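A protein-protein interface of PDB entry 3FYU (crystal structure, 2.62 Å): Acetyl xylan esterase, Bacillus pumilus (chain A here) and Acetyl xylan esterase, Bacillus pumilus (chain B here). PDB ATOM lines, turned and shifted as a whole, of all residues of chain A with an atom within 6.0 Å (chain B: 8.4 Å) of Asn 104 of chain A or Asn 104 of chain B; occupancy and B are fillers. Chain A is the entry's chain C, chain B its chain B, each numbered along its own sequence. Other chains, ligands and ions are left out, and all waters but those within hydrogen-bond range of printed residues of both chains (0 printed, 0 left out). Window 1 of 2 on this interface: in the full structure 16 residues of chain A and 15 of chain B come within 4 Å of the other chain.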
ATOM      1  N   TYR A  49     -24.120  -7.219  12.297  1.00  0.00           N
ATOM      2  CA  TYR A  49     -23.988  -8.238  11.272  1.00  0.00           C
ATOM      3  C   TYR A  49     -25.382  -8.810  11.002  1.00  0.00           C
ATOM      4  O   TYR A  49     -26.122  -9.115  11.936  1.00  0.00           O
ATOM      5  CB  TYR A  49     -23.039  -9.337  11.742  1.00  0.00           C
ATOM      6  CG  TYR A  49     -22.740 -10.367  10.686  1.00  0.00           C
ATOM      7  CD1 TYR A  49     -23.601 -11.444  10.465  1.00  0.00           C
ATOM      8  CD2 TYR A  49     -21.584 -10.268   9.903  1.00  0.00           C
ATOM      9  CE1 TYR A  49     -23.312 -12.402   9.491  1.00  0.00           C
ATOM     10  CE2 TYR A  49     -21.288 -11.213   8.934  1.00  0.00           C
ATOM     11  CZ  TYR A  49     -22.151 -12.277   8.733  1.00  0.00           C
ATOM     12  OH  TYR A  49     -21.831 -13.226   7.791  1.00  0.00           O
ATOM     13  N   ILE A  99     -15.015 -12.900   9.037  1.00  0.00           N
ATOM     14  CA  ILE A  99     -16.212 -12.688   9.845  1.00  0.00           C
ATOM     15  C   ILE A  99     -17.388 -13.618   9.551  1.00  0.00           C
ATOM     16  O   ILE A  99     -18.077 -14.057  10.476  1.00  0.00           O
ATOM     17  CB  ILE A  99     -16.705 -11.235   9.725  1.00  0.00           C
ATOM     18  CG1 ILE A  99     -17.805 -10.977  10.751  1.00  0.00           C
ATOM     19  CG2 ILE A  99     -17.212 -10.962   8.311  1.00  0.00           C
ATOM     20  CD1 ILE A  99     -18.153  -9.519  10.915  1.00  0.00           C
ATOM     21  N   HIS A 100     -17.611 -13.936   8.281  1.00  0.00           N
ATOM     22  CA  HIS A 100     -18.729 -14.787   7.928  1.00  0.00           C
ATOM     23  C   HIS A 100     -18.572 -16.183   8.488  1.00  0.00           C
ATOM     24  O   HIS A 100     -19.550 -16.789   8.907  1.00  0.00           O
ATOM     25  CB  HIS A 100     -18.893 -14.826   6.410  1.00  0.00           C
ATOM     26  CG  HIS A 100     -19.017 -13.469   5.797  1.00  0.00           C
ATOM     27  ND1 HIS A 100     -20.034 -12.598   6.128  1.00  0.00           N
ATOM     28  CD2 HIS A 100     -18.224 -12.808   4.920  1.00  0.00           C
ATOM     29  CE1 HIS A 100     -19.859 -11.456   5.483  1.00  0.00           C
ATOM     30  NE2 HIS A 100     -18.768 -11.558   4.744  1.00  0.00           N
ATOM     31  N   ASP A 101     -17.346 -16.694   8.508  1.00  0.00           N
ATOM     32  CA  ASP A 101     -17.116 -18.034   9.037  1.00  0.00           C
ATOM     33  C   ASP A 101     -17.198 -18.016  10.556  1.00  0.00           C
ATOM     34  O   ASP A 101     -17.709 -18.955  11.176  1.00  0.00           O
ATOM     35  CB  ASP A 101     -15.762 -18.569   8.573  1.00  0.00           C
ATOM     36  CG  ASP A 101     -15.680 -18.674   7.072  1.00  0.00           C
ATOM     37  OD1 ASP A 101     -16.574 -19.325   6.482  1.00  0.00           O
ATOM     38  OD2 ASP A 101     -14.733 -18.102   6.486  1.00  0.00           O
ATOM     39  N   ILE A 102     -16.702 -16.938  11.148  1.00  0.00           N
ATOM     40  CA  ILE A 102     -16.752 -16.783  12.589  1.00  0.00           C
ATOM     41  C   ILE A 102     -18.221 -16.840  13.009  1.00  0.00           C
ATOM     42  O   ILE A 102     -18.575 -17.540  13.959  1.00  0.00           O
ATOM     43  CB  ILE A 102     -16.164 -15.421  13.026  1.00  0.00           C
ATOM     44  CG1 ILE A 102     -14.720 -15.292  12.529  1.00  0.00           C
ATOM     45  CG2 ILE A 102     -16.237 -15.270  14.549  1.00  0.00           C
ATOM     46  CD1 ILE A 102     -13.836 -16.428  12.936  1.00  0.00           C
ATOM     47  N   VAL A 103     -19.076 -16.106  12.300  1.00  0.00           N
ATOM     48  CA  VAL A 103     -20.496 -16.095  12.624  1.00  0.00           C
ATOM     49  C   VAL A 103     -21.107 -17.485  12.498  1.00  0.00           C
ATOM     50  O   VAL A 103     -21.868 -17.916  13.365  1.00  0.00           O
ATOM     51  CB  VAL A 103     -21.262 -15.098  11.730  1.00  0.00           C
ATOM     52  CG1 VAL A 103     -22.769 -15.287  11.892  1.00  0.00           C
ATOM     53  CG2 VAL A 103     -20.870 -13.672  12.105  1.00  0.00           C
ATOM     54  N   ASN A 104     -20.767 -18.198  11.430  1.00  0.00           N
ATOM     55  CA  ASN A 104     -21.298 -19.543  11.245  1.00  0.00           C
ATOM     56  C   ASN A 104     -20.874 -20.471  12.369  1.00  0.00           C
ATOM     57  O   ASN A 104     -21.646 -21.341  12.781  1.00  0.00           O
ATOM     58  CB  ASN A 104     -20.856 -20.131   9.909  1.00  0.00           C
ATOM     59  CG  ASN A 104     -21.514 -19.458   8.750  1.00  0.00           C
ATOM     60  OD1 ASN A 104     -22.571 -18.845   8.900  1.00  0.00           O
ATOM     61  ND2 ASN A 104     -20.909 -19.573   7.575  1.00  0.00           N
ATOM     62  N   TRP A 105     -19.644 -20.302  12.854  1.00  0.00           N
ATOM     63  CA  TRP A 105     -19.166 -21.132  13.952  1.00  0.00           C
ATOM     64  C   TRP A 105     -20.035 -20.865  15.169  1.00  0.00           C
ATOM     65  O   TRP A 105     -20.404 -21.791  15.889  1.00  0.00           O
ATOM     66  CB  TRP A 105     -17.694 -20.843  14.258  1.00  0.00           C
ATOM     67  CG  TRP A 105     -16.749 -21.682  13.428  1.00  0.00           C
ATOM     68  CD1 TRP A 105     -15.779 -21.233  12.581  1.00  0.00           C
ATOM     69  CD2 TRP A 105     -16.709 -23.116  13.357  1.00  0.00           C
ATOM     70  NE1 TRP A 105     -15.141 -22.294  11.981  1.00  0.00           N
ATOM     71  CE2 TRP A 105     -15.691 -23.460  12.441  1.00  0.00           C
ATOM     72  CE3 TRP A 105     -17.433 -24.140  13.981  1.00  0.00           C
ATOM     73  CZ2 TRP A 105     -15.377 -24.785  12.129  1.00  0.00           C
ATOM     74  CZ3 TRP A 105     -17.126 -25.450  13.677  1.00  0.00           C
ATOM     75  CH2 TRP A 105     -16.102 -25.764  12.753  1.00  0.00           C
ATOM     76  N   ALA A 106     -20.382 -19.599  15.383  1.00  0.00           N
ATOM     77  CA  ALA A 106     -21.238 -19.244  16.509  1.00  0.00           C
ATOM     78  C   ALA A 106     -22.627 -19.846  16.297  1.00  0.00           C
ATOM     79  O   ALA A 106     -23.287 -20.224  17.249  1.00  0.00           O
ATOM     80  CB  ALA A 106     -21.334 -17.720  16.652  1.00  0.00           C
ATOM     81  N   LEU A 107     -23.072 -19.933  15.048  1.00  0.00           N
ATOM     82  CA  LEU A 107     -24.381 -20.504  14.770  1.00  0.00           C
ATOM     83  C   LEU A 107     -24.362 -21.989  15.073  1.00  0.00           C
ATOM     84  O   LEU A 107     -25.397 -22.589  15.360  1.00  0.00           O
ATOM     85  CB  LEU A 107     -24.782 -20.262  13.311  1.00  0.00           C
ATOM     86  CG  LEU A 107     -25.255 -18.832  13.022  1.00  0.00           C
ATOM     87  CD1 LEU A 107     -25.427 -18.632  11.541  1.00  0.00           C
ATOM     88  CD2 LEU A 107     -26.560 -18.573  13.753  1.00  0.00           C
ATOM     89  N   HIS A 108     -23.179 -22.584  15.013  1.00  0.00           N
ATOM     90  CA  HIS A 108     -23.035 -23.998  15.311  1.00  0.00           C
ATOM     91  C   HIS A 108     -22.988 -24.195  16.817  1.00  0.00           C
ATOM     92  O   HIS A 108     -22.878 -25.321  17.303  1.00  0.00           O
ATOM     93  CB  HIS A 108     -21.771 -24.538  14.671  1.00  0.00           C
ATOM     94  CG  HIS A 108     -21.939 -24.891  13.229  1.00  0.00           C
ATOM     95  ND1 HIS A 108     -22.204 -26.176  12.805  1.00  0.00           N
ATOM     96  CD2 HIS A 108     -21.927 -24.119  12.116  1.00  0.00           C
ATOM     97  CE1 HIS A 108     -22.350 -26.178  11.492  1.00  0.00           C
ATOM     98  NE2 HIS A 108     -22.187 -24.943  11.051  1.00  0.00           N
ATOM     99  N   GLY A 109     -23.064 -23.082  17.544  1.00  0.00           N
ATOM    100  CA  GLY A 109     -23.051 -23.117  18.994  1.00  0.00           C
ATOM    101  C   GLY A 109     -21.762 -22.725  19.696  1.00  0.00           C
ATOM    102  O   GLY A 109     -21.675 -22.830  20.926  1.00  0.00           O
ATOM    103  N   TYR B  49     -26.203 -35.290  10.310  1.00  0.00           N
ATOM    104  CA  TYR B  49     -25.196 -34.268  10.086  1.00  0.00           C
ATOM    105  C   TYR B  49     -24.785 -33.711  11.451  1.00  0.00           C
ATOM    106  O   TYR B  49     -25.625 -33.417  12.293  1.00  0.00           O
ATOM    107  CB  TYR B  49     -25.762 -33.168   9.181  1.00  0.00           C
ATOM    108  CG  TYR B  49     -24.745 -32.128   8.772  1.00  0.00           C
ATOM    109  CD1 TYR B  49     -24.454 -31.053   9.602  1.00  0.00           C
ATOM    110  CD2 TYR B  49     -24.056 -32.232   7.561  1.00  0.00           C
ATOM    111  CE1 TYR B  49     -23.511 -30.107   9.242  1.00  0.00           C
ATOM    112  CE2 TYR B  49     -23.106 -31.296   7.191  1.00  0.00           C
ATOM    113  CZ  TYR B  49     -22.839 -30.232   8.033  1.00  0.00           C
ATOM    114  OH  TYR B  49     -21.916 -29.276   7.673  1.00  0.00           O
ATOM    115  N   VAL B  51     -24.582 -31.288  13.462  1.00  0.00           N
ATOM    116  CA  VAL B  51     -25.004 -29.919  13.725  1.00  0.00           C
ATOM    117  C   VAL B  51     -26.118 -29.930  14.758  1.00  0.00           C
ATOM    118  O   VAL B  51     -26.846 -30.910  14.892  1.00  0.00           O
ATOM    119  CB  VAL B  51     -25.509 -29.207  12.437  1.00  0.00           C
ATOM    120  CG1 VAL B  51     -26.774 -29.873  11.925  1.00  0.00           C
ATOM    121  CG2 VAL B  51     -25.764 -27.731  12.726  1.00  0.00           C
ATOM    122  N   VAL B  54     -30.613 -27.956  13.779  1.00  0.00           N
ATOM    123  CA  VAL B  54     -31.015 -28.093  12.387  1.00  0.00           C
ATOM    124  C   VAL B  54     -31.253 -29.564  12.035  1.00  0.00           C
ATOM    125  O   VAL B  54     -30.508 -30.450  12.464  1.00  0.00           O
ATOM    126  CB  VAL B  54     -29.933 -27.491  11.419  1.00  0.00           C
ATOM    127  CG1 VAL B  54     -30.210 -27.899   9.968  1.00  0.00           C
ATOM    128  CG2 VAL B  54     -29.927 -25.973  11.533  1.00  0.00           C
ATOM    129  N   VAL B  56     -31.564 -32.171   8.917  1.00  0.00           N
ATOM    130  CA  VAL B  56     -31.208 -32.286   7.517  1.00  0.00           C
ATOM    131  C   VAL B  56     -31.917 -33.469   6.880  1.00  0.00           C
ATOM    132  O   VAL B  56     -32.133 -34.499   7.516  1.00  0.00           O
ATOM    133  CB  VAL B  56     -29.678 -32.456   7.361  1.00  0.00           C
ATOM    134  CG1 VAL B  56     -29.294 -32.563   5.880  1.00  0.00           C
ATOM    135  CG2 VAL B  56     -28.966 -31.283   8.036  1.00  0.00           C
ATOM    136  N   ALA B  74     -32.229 -28.641   4.565  1.00  0.00           N
ATOM    137  CA  ALA B  74     -31.991 -28.384   5.982  1.00  0.00           C
ATOM    138  C   ALA B  74     -33.062 -27.450   6.506  1.00  0.00           C
ATOM    139  O   ALA B  74     -33.432 -26.481   5.843  1.00  0.00           O
ATOM    140  CB  ALA B  74     -30.602 -27.770   6.195  1.00  0.00           C
ATOM    141  N   PRO B  76     -34.488 -25.306  10.105  1.00  0.00           N
ATOM    142  CA  PRO B  76     -34.157 -24.890  11.465  1.00  0.00           C
ATOM    143  C   PRO B  76     -34.949 -25.828  12.367  1.00  0.00           C
ATOM    144  O   PRO B  76     -36.106 -26.126  12.079  1.00  0.00           O
ATOM    145  CB  PRO B  76     -34.687 -23.462  11.526  1.00  0.00           C
ATOM    146  CG  PRO B  76     -34.528 -22.986  10.129  1.00  0.00           C
ATOM    147  CD  PRO B  76     -34.993 -24.173   9.315  1.00  0.00           C
ATOM    148  N   LEU B  85     -35.328 -21.065   1.309  1.00  0.00           N
ATOM    149  CA  LEU B  85     -34.411 -20.719   0.242  1.00  0.00           C
ATOM    150  C   LEU B  85     -34.173 -21.915  -0.662  1.00  0.00           C
ATOM    151  O   LEU B  85     -34.029 -23.043  -0.193  1.00  0.00           O
ATOM    152  CB  LEU B  85     -33.060 -20.285   0.802  1.00  0.00           C
ATOM    153  CG  LEU B  85     -32.968 -19.022   1.653  1.00  0.00           C
ATOM    154  CD1 LEU B  85     -31.553 -18.894   2.191  1.00  0.00           C
ATOM    155  CD2 LEU B  85     -33.346 -17.807   0.830  1.00  0.00           C
ATOM    156  N   GLY B  98     -23.055 -29.633  -1.649  1.00  0.00           N
ATOM    157  CA  GLY B  98     -22.975 -28.350  -0.961  1.00  0.00           C
ATOM    158  C   GLY B  98     -23.699 -28.379   0.372  1.00  0.00           C
ATOM    159  O   GLY B  98     -24.184 -27.353   0.861  1.00  0.00           O
ATOM    160  N   ILE B  99     -23.751 -29.563   0.975  1.00  0.00           N
ATOM    161  CA  ILE B  99     -24.448 -29.775   2.246  1.00  0.00           C
ATOM    162  C   ILE B  99     -24.059 -28.845   3.391  1.00  0.00           C
ATOM    163  O   ILE B  99     -24.917 -28.390   4.143  1.00  0.00           O
ATOM    164  CB  ILE B  99     -24.291 -31.236   2.706  1.00  0.00           C
ATOM    165  CG1 ILE B  99     -25.224 -31.507   3.883  1.00  0.00           C
ATOM    166  CG2 ILE B  99     -22.830 -31.522   3.052  1.00  0.00           C
ATOM    167  CD1 ILE B  99     -25.344 -32.961   4.207  1.00  0.00           C
ATOM    168  N   HIS B 100     -22.775 -28.556   3.524  1.00  0.00           N
ATOM    169  CA  HIS B 100     -22.316 -27.684   4.590  1.00  0.00           C
ATOM    170  C   HIS B 100     -22.887 -26.270   4.479  1.00  0.00           C
ATOM    171  O   HIS B 100     -23.203 -25.633   5.484  1.00  0.00           O
ATOM    172  CB  HIS B 100     -20.790 -27.640   4.600  1.00  0.00           C
ATOM    173  CG  HIS B 100     -20.157 -28.990   4.656  1.00  0.00           C
ATOM    174  ND1 HIS B 100     -20.328 -29.845   5.725  1.00  0.00           N
ATOM    175  CD2 HIS B 100     -19.403 -29.660   3.752  1.00  0.00           C
ATOM    176  CE1 HIS B 100     -19.708 -30.985   5.475  1.00  0.00           C
ATOM    177  NE2 HIS B 100     -19.141 -30.899   4.285  1.00  0.00           N
ATOM    178  N   ASP B 101     -23.024 -25.769   3.258  1.00  0.00           N
ATOM    179  CA  ASP B 101     -23.567 -24.429   3.085  1.00  0.00           C
ATOM    180  C   ASP B 101     -25.080 -24.453   3.299  1.00  0.00           C
ATOM    181  O   ASP B 101     -25.646 -23.509   3.852  1.00  0.00           O
ATOM    182  CB  ASP B 101     -23.204 -23.885   1.700  1.00  0.00           C
ATOM    183  CG  ASP B 101     -21.709 -23.775   1.501  1.00  0.00           C
ATOM    184  OD1 ASP B 101     -21.050 -23.156   2.360  1.00  0.00           O
ATOM    185  OD2 ASP B 101     -21.186 -24.305   0.497  1.00  0.00           O
ATOM    186  N   ILE B 102     -25.723 -25.540   2.871  1.00  0.00           N
ATOM    187  CA  ILE B 102     -27.163 -25.699   3.043  1.00  0.00           C
ATOM    188  C   ILE B 102     -27.455 -25.663   4.542  1.00  0.00           C
ATOM    189  O   ILE B 102     -28.368 -24.974   4.997  1.00  0.00           O
ATOM    190  CB  ILE B 102     -27.659 -27.057   2.482  1.00  0.00           C
ATOM    191  CG1 ILE B 102     -27.240 -27.206   1.015  1.00  0.00           C
ATOM    192  CG2 ILE B 102     -29.171 -27.180   2.653  1.00  0.00           C
ATOM    193  CD1 ILE B 102     -27.701 -26.089   0.136  1.00  0.00           C
ATOM    194  N   VAL B 103     -26.668 -26.405   5.314  1.00  0.00           N
ATOM    195  CA  VAL B 103     -26.863 -26.418   6.756  1.00  0.00           C
ATOM    196  C   VAL B 103     -26.669 -25.031   7.358  1.00  0.00           C
ATOM    197  O   VAL B 103     -27.448 -24.605   8.207  1.00  0.00           O
ATOM    198  CB  VAL B 103     -25.911 -27.419   7.445  1.00  0.00           C
ATOM    199  CG1 VAL B 103     -25.964 -27.230   8.962  1.00  0.00           C
ATOM    200  CG2 VAL B 103     -26.319 -28.860   7.072  1.00  0.00           C
ATOM    201  N   ASN B 104     -25.644 -24.316   6.914  1.00  0.00           N
ATOM    202  CA  ASN B 104     -25.412 -22.985   7.451  1.00  0.00           C
ATOM    203  C   ASN B 104     -26.574 -22.070   7.119  1.00  0.00           C
ATOM    204  O   ASN B 104     -26.944 -21.219   7.915  1.00  0.00           O
ATOM    205  CB  ASN B 104     -24.100 -22.387   6.915  1.00  0.00           C
ATOM    206  CG  ASN B 104     -22.876 -23.097   7.456  1.00  0.00           C
ATOM    207  OD1 ASN B 104     -22.920 -23.689   8.528  1.00  0.00           O
ATOM    208  ND2 ASN B 104     -21.768 -23.028   6.723  1.00  0.00           N
ATOM    209  N   TRP B 105     -27.147 -22.225   5.937  1.00  0.00           N
ATOM    210  CA  TRP B 105     -28.274 -21.378   5.583  1.00  0.00           C
ATOM    211  C   TRP B 105     -29.409 -21.642   6.569  1.00  0.00           C
ATOM    212  O   TRP B 105     -30.115 -20.718   6.986  1.00  0.00           O
ATOM    213  CB  TRP B 105     -28.730 -21.651   4.139  1.00  0.00           C
ATOM    214  CG  TRP B 105     -28.005 -20.820   3.128  1.00  0.00           C
ATOM    215  CD1 TRP B 105     -27.245 -21.269   2.088  1.00  0.00           C
ATOM    216  CD2 TRP B 105     -27.941 -19.390   3.084  1.00  0.00           C
ATOM    217  NE1 TRP B 105     -26.709 -20.212   1.399  1.00  0.00           N
ATOM    218  CE2 TRP B 105     -27.116 -19.043   1.989  1.00  0.00           C
ATOM    219  CE3 TRP B 105     -28.498 -18.365   3.866  1.00  0.00           C
ATOM    220  CZ2 TRP B 105     -26.827 -17.707   1.652  1.00  0.00           C
ATOM    221  CZ3 TRP B 105     -28.214 -17.037   3.532  1.00  0.00           C
ATOM    222  CH2 TRP B 105     -27.381 -16.724   2.428  1.00  0.00           C
ATOM    223  N   ALA B 106     -29.571 -22.906   6.951  1.00  0.00           N
ATOM    224  CA  ALA B 106     -30.629 -23.271   7.889  1.00  0.00           C
ATOM    225  C   ALA B 106     -30.328 -22.672   9.247  1.00  0.00           C
ATOM    226  O   ALA B 106     -31.237 -22.265   9.956  1.00  0.00           O
ATOM    227  CB  ALA B 106     -30.765 -24.791   7.987  1.00  0.00           C
ATOM    228  N   LEU B 107     -29.047 -22.610   9.602  1.00  0.00           N
ATOM    229  CA  LEU B 107     -28.639 -22.026  10.875  1.00  0.00           C
ATOM    230  C   LEU B 107     -28.927 -20.532  10.871  1.00  0.00           C
ATOM    231  O   LEU B 107     -29.105 -19.921  11.916  1.00  0.00           O
ATOM    232  CB  LEU B 107     -27.151 -22.279  11.134  1.00  0.00           C
ATOM    233  CG  LEU B 107     -26.799 -23.715  11.555  1.00  0.00           C
ATOM    234  CD1 LEU B 107     -25.287 -23.912  11.564  1.00  0.00           C
ATOM    235  CD2 LEU B 107     -27.409 -24.002  12.925  1.00  0.00           C
ATOM    236  N   HIS B 108     -28.974 -19.942   9.683  1.00  0.00           N
ATOM    237  CA  HIS B 108     -29.287 -18.526   9.566  1.00  0.00           C
ATOM    238  C   HIS B 108     -30.792 -18.340   9.664  1.00  0.00           C
ATOM    239  O   HIS B 108     -31.283 -17.212   9.627  1.00  0.00           O
ATOM    240  CB  HIS B 108     -28.766 -17.969   8.246  1.00  0.00           C
ATOM    241  CG  HIS B 108     -27.312 -17.614   8.283  1.00  0.00           C
ATOM    242  ND1 HIS B 108     -26.866 -16.333   8.521  1.00  0.00           N
ATOM    243  CD2 HIS B 108     -26.203 -18.383   8.153  1.00  0.00           C
ATOM    244  CE1 HIS B 108     -25.544 -16.327   8.534  1.00  0.00           C
ATOM    245  NE2 HIS B 108     -25.118 -17.559   8.315  1.00  0.00           N
ATOM    246  N   GLY B 109     -31.514 -19.458   9.794  1.00  0.00           N
ATOM    247  CA  GLY B 109     -32.958 -19.419   9.930  1.00  0.00           C
ATOM    248  C   GLY B 109     -33.763 -19.775   8.695  1.00  0.00           C
ATOM    249  O   GLY B 109     -34.979 -19.608   8.689  1.00  0.00           O
ATOM    250  N   TYR B 110     -33.114 -20.284   7.654  1.00  0.00           N
ATOM    251  CA  TYR B 110     -33.832 -20.617   6.428  1.00  0.00           C
ATOM    252  C   TYR B 110     -33.969 -22.100   6.126  1.00  0.00           C
ATOM    253  O   TYR B 110     -32.988 -22.836   6.120  1.00  0.00           O
ATOM    254  CB  TYR B 110     -33.148 -19.967   5.225  1.00  0.00           C
ATOM    255  CG  TYR B 110     -32.988 -18.477   5.328  1.00  0.00           C
ATOM    256  CD1 TYR B 110     -34.028 -17.623   4.990  1.00  0.00           C
ATOM    257  CD2 TYR B 110     -31.796 -17.921   5.775  1.00  0.00           C
ATOM    258  CE1 TYR B 110     -33.885 -16.241   5.093  1.00  0.00           C
ATOM    259  CE2 TYR B 110     -31.645 -16.547   5.886  1.00  0.00           C
ATOM    260  CZ  TYR B 110     -32.692 -15.712   5.543  1.00  0.00           C
ATOM    261  OH  TYR B 110     -32.558 -14.352   5.662  1.00  0.00           O
ATOM    262  N   THR B 112     -33.662 -24.541   3.921  1.00  0.00           N
ATOM    263  CA  THR B 112     -32.955 -24.510   2.641  1.00  0.00           C
ATOM    264  C   THR B 112     -32.811 -25.829   1.873  1.00  0.00           C
ATOM    265  O   THR B 112     -32.493 -26.880   2.440  1.00  0.00           O
ATOM    266  CB  THR B 112     -31.556 -23.924   2.837  1.00  0.00           C
ATOM    267  OG1 THR B 112     -31.658 -22.695   3.560  1.00  0.00           O
ATOM    268  CG2 THR B 112     -30.902 -23.657   1.505  1.00  0.00           C
ATOM    269  N   PHE B 300     -16.043 -16.156  -4.460  1.00  0.00           N
ATOM    270  CA  PHE B 300     -16.776 -15.698  -3.294  1.00  0.00           C
ATOM    271  C   PHE B 300     -16.318 -14.268  -2.987  1.00  0.00           C
ATOM    272  O   PHE B 300     -15.130 -14.001  -2.886  1.00  0.00           O
ATOM    273  CB  PHE B 300     -16.476 -16.602  -2.099  1.00  0.00           C
ATOM    274  CG  PHE B 300     -17.046 -16.101  -0.790  1.00  0.00           C
ATOM    275  CD1 PHE B 300     -18.408 -16.155  -0.547  1.00  0.00           C
ATOM    276  CD2 PHE B 300     -16.215 -15.580   0.195  1.00  0.00           C
ATOM    277  CE1 PHE B 300     -18.946 -15.700   0.661  1.00  0.00           C
ATOM    278  CE2 PHE B 300     -16.735 -15.121   1.401  1.00  0.00           C
ATOM    279  CZ  PHE B 300     -18.107 -15.179   1.636  1.00  0.00           C
ATOM    280  N   GLN B 305     -21.462 -11.058   0.605  1.00  0.00           N
ATOM    281  CA  GLN B 305     -22.122 -12.000   1.514  1.00  0.00           C
ATOM    282  C   GLN B 305     -22.940 -11.200   2.523  1.00  0.00           C
ATOM    283  O   GLN B 305     -24.079 -11.550   2.833  1.00  0.00           O
ATOM    284  CB  GLN B 305     -21.100 -12.864   2.247  1.00  0.00           C
ATOM    285  CG  GLN B 305     -21.716 -13.992   3.068  1.00  0.00           C
ATOM    286  CD  GLN B 305     -22.498 -14.999   2.221  1.00  0.00           C
ATOM    287  OE1 GLN B 305     -22.477 -14.956   0.984  1.00  0.00           O
ATOM    288  NE2 GLN B 305     -23.182 -15.921   2.891  1.00  0.00           N
ATOM    289  N   LEU B 309     -26.849 -11.571   2.960  1.00  0.00           N
ATOM    290  CA  LEU B 309     -27.476 -11.910   4.234  1.00  0.00           C
ATOM    291  C   LEU B 309     -28.420 -10.809   4.684  1.00  0.00           C
ATOM    292  O   LEU B 309     -29.499 -11.069   5.222  1.00  0.00           O
ATOM    293  CB  LEU B 309     -26.413 -12.131   5.305  1.00  0.00           C
ATOM    294  CG  LEU B 309     -25.533 -13.360   5.096  1.00  0.00           C
ATOM    295  CD1 LEU B 309     -24.416 -13.392   6.133  1.00  0.00           C
ATOM    296  CD2 LEU B 309     -26.402 -14.602   5.188  1.00  0.00           C
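NE2 of His 108 of chain A is in hydrogen-bond range of OD1 of Asn 104 of chain B (2.9 Å).
OD1 of Asn 104 of chain A sits at hydrogen-bond distance from NE2 of His 108 of chain B, at 2.9 Å.
Printed residues of chain A that touch a printed residue of chain B: Tyr 49, His 100, Asn 104, Leu 107 and His 108.
ND2 of Asn 104 of chain B is in hydrogen-bond range of O of His 100 of chain B (3.2 Å).
ND1 of His 100 of chain A is in hydrogen-bond range of OH of Tyr 49 of chain A (2.5 Å).
The side-chain amide nitrogen of Asn 104 of chain A sits close to the backbone carbonyl oxygen of His 100 of chain A (3.4 Å).
Among the printed residues, merely in contact across the chains: Tyr 49 of chain A with Leu 309 of chain B, His 100 of chain A with Gln 305 of chain B, Asn 104 of chain A with Asn 104 of chain B, Leu 107 of chain A with Leu 107 of chain B, Leu 107 of chain A with His 108 of chain B, His 108 of chain A with Val 51 of chain B and His 108 of chain A with Leu 107 of chain B.
Asn 104 of chain A touches just these residues of chain B: Asn 104 (3.7 Å) and His 108 (2.9 Å).
Of chain A, only Asn 104 (3.7 Å) and His 108 (2.9 Å) come within 4 Å of Asn 104 of chain B.
Of the printed residues of chain A, Val 51 of chain B touches His 108 (3.9 Å).
Of the printed residues of chain A, Gln 305 of chain B touches His 100.
Ile 102 of chain B touches none of the printed residues of chain A.
The nearest printed residue of chain A that does not touch Val 51 of chain B is Leu 107 of chain A (5.8 Å).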
